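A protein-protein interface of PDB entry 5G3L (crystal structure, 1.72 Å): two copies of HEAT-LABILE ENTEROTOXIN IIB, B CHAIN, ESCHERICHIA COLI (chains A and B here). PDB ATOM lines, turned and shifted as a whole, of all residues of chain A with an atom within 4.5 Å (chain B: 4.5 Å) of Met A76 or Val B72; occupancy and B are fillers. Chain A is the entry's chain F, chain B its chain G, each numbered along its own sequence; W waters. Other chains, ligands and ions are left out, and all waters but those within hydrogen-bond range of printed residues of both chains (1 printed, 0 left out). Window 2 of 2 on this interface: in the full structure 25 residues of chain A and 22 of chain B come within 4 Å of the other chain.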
ATOM      1  N   VAL A  21      23.293 -12.638  23.898  1.00  0.00           N
ATOM      2  CA  VAL A  21      23.351 -11.980  22.588  1.00  0.00           C
ATOM      3  C   VAL A  21      22.887 -12.946  21.476  1.00  0.00           C
ATOM      4  O   VAL A  21      23.370 -14.072  21.385  1.00  0.00           O
ATOM      5  CB  VAL A  21      24.763 -11.451  22.288  1.00  0.00           C
ATOM      6  CG1 VAL A  21      24.835 -10.718  20.944  1.00  0.00           C
ATOM      7  CG2 VAL A  21      25.241 -10.526  23.390  1.00  0.00           C
ATOM      8  N   ALA A  71      26.093 -20.112  16.017  1.00  0.00           N
ATOM      9  CA  ALA A  71      25.104 -19.197  16.615  1.00  0.00           C
ATOM     10  C   ALA A  71      24.238 -18.556  15.548  1.00  0.00           C
ATOM     11  O   ALA A  71      23.013 -18.446  15.706  1.00  0.00           O
ATOM     12  CB  ALA A  71      25.798 -18.131  17.444  1.00  0.00           C
ATOM     13  N   SER A  74      21.839 -21.278  13.973  1.00  0.00           N
ATOM     14  CA  SER A  74      20.884 -21.915  14.907  1.00  0.00           C
ATOM     15  C   SER A  74      20.011 -20.927  15.674  1.00  0.00           C
ATOM     16  O   SER A  74      18.951 -21.309  16.173  1.00  0.00           O
ATOM     17  CB  SER A  74      21.623 -22.777  15.907  1.00  0.00           C
ATOM     18  OG  SER A  74      22.381 -21.969  16.837  1.00  0.00           O
ATOM     19  N   GLY A  75      20.461 -19.686  15.789  1.00  0.00           N
ATOM     20  CA  GLY A  75      19.823 -18.717  16.714  1.00  0.00           C
ATOM     21  C   GLY A  75      20.135 -18.944  18.201  1.00  0.00           C
ATOM     22  O   GLY A  75      19.604 -18.244  19.049  1.00  0.00           O
ATOM     23  N   MET A  76      21.053 -19.855  18.522  1.00  0.00           N
ATOM     24  CA  MET A  76      21.552 -20.014  19.884  1.00  0.00           C
ATOM     25  C   MET A  76      22.265 -18.757  20.347  1.00  0.00           C
ATOM     26  O   MET A  76      23.006 -18.152  19.581  1.00  0.00           O
ATOM     27  CB  MET A  76      22.558 -21.174  19.989  1.00  0.00           C
ATOM     28  CG  MET A  76      21.913 -22.522  20.037  1.00  0.00           C
ATOM     29  SD  MET A  76      23.160 -23.845  20.278  1.00  0.00           S
ATOM     30  CE  MET A  76      22.038 -25.228  20.454  1.00  0.00           C
ATOM     31  N   ARG A  77      22.047 -18.377  21.595  1.00  0.00           N
ATOM     32  CA  ARG A  77      22.639 -17.191  22.150  1.00  0.00           C
ATOM     33  C   ARG A  77      24.097 -17.415  22.534  1.00  0.00           C
ATOM     34  O   ARG A  77      24.526 -18.550  22.758  1.00  0.00           O
ATOM     35  CB  ARG A  77      21.855 -16.734  23.374  1.00  0.00           C
ATOM     36  CG  ARG A  77      20.356 -16.650  23.110  1.00  0.00           C
ATOM     37  CD  ARG A  77      19.868 -15.262  22.984  1.00  0.00           C
ATOM     38  NE  ARG A  77      18.619 -15.150  22.209  1.00  0.00           N
ATOM     39  CZ  ARG A  77      17.897 -14.034  22.116  1.00  0.00           C
ATOM     40  NH1 ARG A  77      18.253 -12.925  22.771  1.00  0.00           N
ATOM     41  NH2 ARG A  77      16.811 -14.019  21.349  1.00  0.00           N
ATOM     42  N   VAL A  78      24.838 -16.328  22.594  1.00  0.00           N
ATOM     43  CA  VAL A  78      26.194 -16.334  23.117  1.00  0.00           C
ATOM     44  C   VAL A  78      26.347 -15.314  24.289  1.00  0.00           C
ATOM     45  O   VAL A  78      25.646 -14.295  24.373  1.00  0.00           O
ATOM     46  CB  VAL A  78      27.257 -16.009  22.045  1.00  0.00           C
ATOM     47  CG1 VAL A  78      27.157 -17.038  20.914  1.00  0.00           C
ATOM     48  CG2 VAL A  78      27.085 -14.610  21.510  1.00  0.00           C
ATOM     49  N   LEU A  96      29.062 -20.243  23.914  1.00  0.00           N
ATOM     50  CA  LEU A  96      27.851 -20.649  23.179  1.00  0.00           C
ATOM     51  C   LEU A  96      26.914 -21.391  24.099  1.00  0.00           C
ATOM     52  O   LEU A  96      27.354 -22.296  24.819  1.00  0.00           O
ATOM     53  CB  LEU A  96      28.212 -21.608  22.045  1.00  0.00           C
ATOM     54  CG  LEU A  96      27.085 -22.129  21.150  1.00  0.00           C
ATOM     55  CD1 LEU A  96      26.438 -21.035  20.353  1.00  0.00           C
ATOM     56  CD2 LEU A  96      27.655 -23.198  20.208  1.00  0.00           C
ATOM     57  N   GLU A  97      25.620 -21.022  24.105  1.00  0.00           N
ATOM     58  CA  GLU A  97      24.714 -21.749  24.992  1.00  0.00           C
ATOM     59  C   GLU A  97      23.549 -22.387  24.307  1.00  0.00           C
ATOM     60  O   GLU A  97      22.886 -21.779  23.454  1.00  0.00           O
ATOM     61  CB  GLU A  97      24.321 -20.933  26.253  1.00  0.00           C
ATOM     62  CG  GLU A  97      23.901 -19.566  26.038  1.00  0.00           C
ATOM     63  CD  GLU A  97      23.372 -18.900  27.340  1.00  0.00           C
ATOM     64  OE1 GLU A  97      24.020 -18.603  28.369  1.00  0.00           O
ATOM     65  OE2 GLU A  97      22.217 -18.617  27.210  1.00  0.00           O
ATOM     66  N   ALA A  98      23.271 -23.625  24.719  1.00  0.00           N
ATOM     67  CA  ALA A  98      22.118 -24.348  24.198  1.00  0.00           C
ATOM     68  C   ALA A  98      20.816 -23.812  24.819  1.00  0.00           C
ATOM     69  O   ALA A  98      20.767 -23.294  25.926  1.00  0.00           O
ATOM     70  CB  ALA A  98      22.254 -25.822  24.467  1.00  0.00           C
ATOM     71  N   LEU B  23      25.928 -31.474  27.932  1.00  0.00           N
ATOM     72  CA  LEU B  23      26.706 -30.270  27.806  1.00  0.00           C
ATOM     73  C   LEU B  23      25.815 -29.197  27.216  1.00  0.00           C
ATOM     74  O   LEU B  23      25.227 -29.409  26.158  1.00  0.00           O
ATOM     75  CB  LEU B  23      27.957 -30.477  26.903  1.00  0.00           C
ATOM     76  CG  LEU B  23      28.898 -31.576  27.412  1.00  0.00           C
ATOM     77  CD1 LEU B  23      30.083 -31.684  26.439  1.00  0.00           C
ATOM     78  CD2 LEU B  23      29.418 -31.286  28.805  1.00  0.00           C
ATOM     79  N   THR B  24      25.771 -28.061  27.903  1.00  0.00           N
ATOM     80  CA  THR B  24      24.928 -26.946  27.490  1.00  0.00           C
ATOM     81  C   THR B  24      25.648 -25.672  27.113  1.00  0.00           C
ATOM     82  O   THR B  24      25.023 -24.748  26.582  1.00  0.00           O
ATOM     83  CB  THR B  24      23.894 -26.628  28.600  1.00  0.00           C
ATOM     84  OG1 THR B  24      24.542 -26.285  29.815  1.00  0.00           O
ATOM     85  CG2 THR B  24      22.968 -27.856  28.828  1.00  0.00           C
ATOM     86  N   LYS B  25      26.916 -25.577  27.460  1.00  0.00           N
ATOM     87  CA  LYS B  25      27.751 -24.446  27.059  1.00  0.00           C
ATOM     88  C   LYS B  25      29.161 -24.872  26.560  1.00  0.00           C
ATOM     89  O   LYS B  25      29.733 -25.831  27.046  1.00  0.00           O
ATOM     90  CB  LYS B  25      27.926 -23.450  28.224  1.00  0.00           C
ATOM     91  CG  LYS B  25      26.586 -23.083  28.880  1.00  0.00           C
ATOM     92  CD  LYS B  25      26.664 -21.850  29.732  1.00  0.00           C
ATOM     93  CE  LYS B  25      25.478 -21.685  30.655  1.00  0.00           C
ATOM     94  NZ  LYS B  25      24.285 -21.208  29.949  1.00  0.00           N
ATOM     95  N   TYR B  26      29.663 -24.097  25.596  1.00  0.00           N
ATOM     96  CA  TYR B  26      30.970 -24.319  24.996  1.00  0.00           C
ATOM     97  C   TYR B  26      31.714 -22.989  24.975  1.00  0.00           C
ATOM     98  O   TYR B  26      31.184 -22.003  24.468  1.00  0.00           O
ATOM     99  CB  TYR B  26      30.798 -24.861  23.585  1.00  0.00           C
ATOM    100  CG  TYR B  26      32.058 -25.226  22.809  1.00  0.00           C
ATOM    101  CD1 TYR B  26      33.005 -26.131  23.333  1.00  0.00           C
ATOM    102  CD2 TYR B  26      32.287 -24.725  21.561  1.00  0.00           C
ATOM    103  CE1 TYR B  26      34.123 -26.487  22.630  1.00  0.00           C
ATOM    104  CE2 TYR B  26      33.408 -25.110  20.843  1.00  0.00           C
ATOM    105  CZ  TYR B  26      34.309 -25.997  21.376  1.00  0.00           C
ATOM    106  OH  TYR B  26      35.438 -26.401  20.663  1.00  0.00           O
ATOM    107  N   ALA B  68      32.449 -31.966  21.527  1.00  0.00           N
ATOM    108  CA  ALA B  68      31.864 -30.948  22.455  1.00  0.00           C
ATOM    109  C   ALA B  68      30.867 -30.050  21.757  1.00  0.00           C
ATOM    110  O   ALA B  68      29.737 -29.867  22.233  1.00  0.00           O
ATOM    111  CB  ALA B  68      32.969 -30.112  23.056  1.00  0.00           C
ATOM    112  N   MET B  69      31.228 -29.529  20.582  1.00  0.00           N
ATOM    113  CA  MET B  69      30.294 -28.676  19.852  1.00  0.00           C
ATOM    114  C   MET B  69      29.063 -29.467  19.428  1.00  0.00           C
ATOM    115  O   MET B  69      27.934 -28.981  19.500  1.00  0.00           O
ATOM    116  CB  MET B  69      30.931 -28.077  18.604  1.00  0.00           C
ATOM    117  CG  MET B  69      29.934 -27.338  17.707  1.00  0.00           C
ATOM    118  SD  MET B  69      29.740 -25.623  18.192  1.00  0.00           S
ATOM    119  CE  MET B  69      31.400 -25.149  17.619  1.00  0.00           C
ATOM    120  N   ALA B  70      29.272 -30.673  18.921  1.00  0.00           N
ATOM    121  CA  ALA B  70      28.152 -31.488  18.451  1.00  0.00           C
ATOM    122  C   ALA B  70      27.173 -31.842  19.584  1.00  0.00           C
ATOM    123  O   ALA B  70      25.948 -31.860  19.359  1.00  0.00           O
ATOM    124  CB  ALA B  70      28.609 -32.765  17.792  1.00  0.00           C
ATOM    125  N   ALA B  71      27.732 -32.085  20.760  1.00  0.00           N
ATOM    126  CA  ALA B  71      26.892 -32.336  21.953  1.00  0.00           C
ATOM    127  C   ALA B  71      26.072 -31.109  22.362  1.00  0.00           C
ATOM    128  O   ALA B  71      24.885 -31.239  22.690  1.00  0.00           O
ATOM    129  CB  ALA B  71      27.764 -32.783  23.142  1.00  0.00           C
ATOM    130  N   VAL B  72      26.706 -29.942  22.331  1.00  0.00           N
ATOM    131  CA  VAL B  72      26.009 -28.676  22.695  1.00  0.00           C
ATOM    132  C   VAL B  72      24.895 -28.403  21.704  1.00  0.00           C
ATOM    133  O   VAL B  72      23.743 -28.078  22.095  1.00  0.00           O
ATOM    134  CB  VAL B  72      26.983 -27.491  22.872  1.00  0.00           C
ATOM    135  CG1 VAL B  72      26.234 -26.175  22.995  1.00  0.00           C
ATOM    136  CG2 VAL B  72      27.851 -27.712  24.105  1.00  0.00           C
ATOM    137  N   LEU B  73      25.161 -28.592  20.418  1.00  0.00           N
ATOM    138  CA  LEU B  73      24.146 -28.312  19.371  1.00  0.00           C
ATOM    139  C   LEU B  73      22.949 -29.249  19.391  1.00  0.00           C
ATOM    140  O   LEU B  73      21.839 -28.820  19.172  1.00  0.00           O
ATOM    141  CB  LEU B  73      24.799 -28.290  17.994  1.00  0.00           C
ATOM    142  CG  LEU B  73      25.711 -27.045  17.788  1.00  0.00           C
ATOM    143  CD1 LEU B  73      26.276 -27.180  16.387  1.00  0.00           C
ATOM    144  CD2 LEU B  73      25.091 -25.632  17.972  1.00  0.00           C
ATOM    145  N   SER B  74      23.182 -30.506  19.716  1.00  0.00           N
ATOM    146  CA  SER B  74      22.221 -31.600  19.543  1.00  0.00           C
ATOM    147  C   SER B  74      21.535 -32.040  20.855  1.00  0.00           C
ATOM    148  O   SER B  74      20.474 -32.660  20.811  1.00  0.00           O
ATOM    149  CB  SER B  74      22.859 -32.830  18.946  1.00  0.00           C
ATOM    150  OG  SER B  74      23.798 -33.451  19.859  1.00  0.00           O
ATOM    151  N   GLY B  75      22.171 -31.746  21.965  1.00  0.00           N
ATOM    152  CA  GLY B  75      21.747 -32.290  23.272  1.00  0.00           C
ATOM    153  C   GLY B  75      22.144 -33.728  23.497  1.00  0.00           C
ATOM    154  O   GLY B  75      21.735 -34.322  24.491  1.00  0.00           O
HETATM  155  O   HOH W   1      22.910 -23.083  28.318  1.00  0.00           O
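CE of Met A76 touches O of Val B72, 3.7 Å away.
CD2 of Leu B73 touches SD of Met A76 (3.5 Å).
O of Leu A96 touches O of Thr B24, 3.8 Å away.
O of Leu A96 touches CA of Lys B25, 3.1 Å away.
Met B69 touches Leu A96 (SD to CD2, 3.8 Å).
Glu A97 touches Thr B24 (CA to O, 3.4 Å).
CB of Ala A98 touches O of Val B72 (3.6 Å).
The backbone NH of Leu A96 is in hydrogen-bond range of the backbone carbonyl oxygen of Tyr B26.
The side-chain carboxylate (OE1) of Glu A97 lies within salt-bridge range of the side-chain amino group (NZ) of Lys B25, 3.1 Å away.
The backbone NH (N) of Ala A98 is in hydrogen-bond range of the backbone carbonyl oxygen (O) of Thr B24.
The side-chain hydroxyl (OG) of Ser A74 is in hydrogen-bond range of the backbone NH (N) of Met A76.
The backbone carbonyl oxygen of Arg A77 lies within hydrogen-bond range of the backbone NH of Glu A97, 3.0 Å away.
Positions printed for both chains: 71, 74 and 75.
Water W1 lies within hydrogen-bond range of the side-chain amino group of Lys B25 (2.8 Å), the backbone carbonyl oxygen of Thr B24 (3.2 Å) and the backbone carbonyl oxygen of Ala A98 (3.2 Å).
Of chain B, only Val B72 and Leu B73 come within 4 Å of Met A76.
Printed residues of chain B within 4 Å of Leu A96: Thr B24 (3.8 Å), Lys B25 (3.1 Å), Tyr B26 (2.8 Å) and Met B69 (3.8 Å).
Of the printed residues of chain A, Tyr B26 touches Leu A96 (2.8 Å).
Of chain A, only Met A76 and Ala A98 come within 4 Å of Val B72.
Printed residues of chain A within 4 Å of Leu B73: Met A76 (3.5 Å).
Of the 12 printed residues of chain B, 6 touch a printed residue of chain A.
Among the printed residues, Asp or Glu carboxylates within 4 Å of a Lys or Arg side-chain nitrogen of the other chain: Glu A97 with Lys B25.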
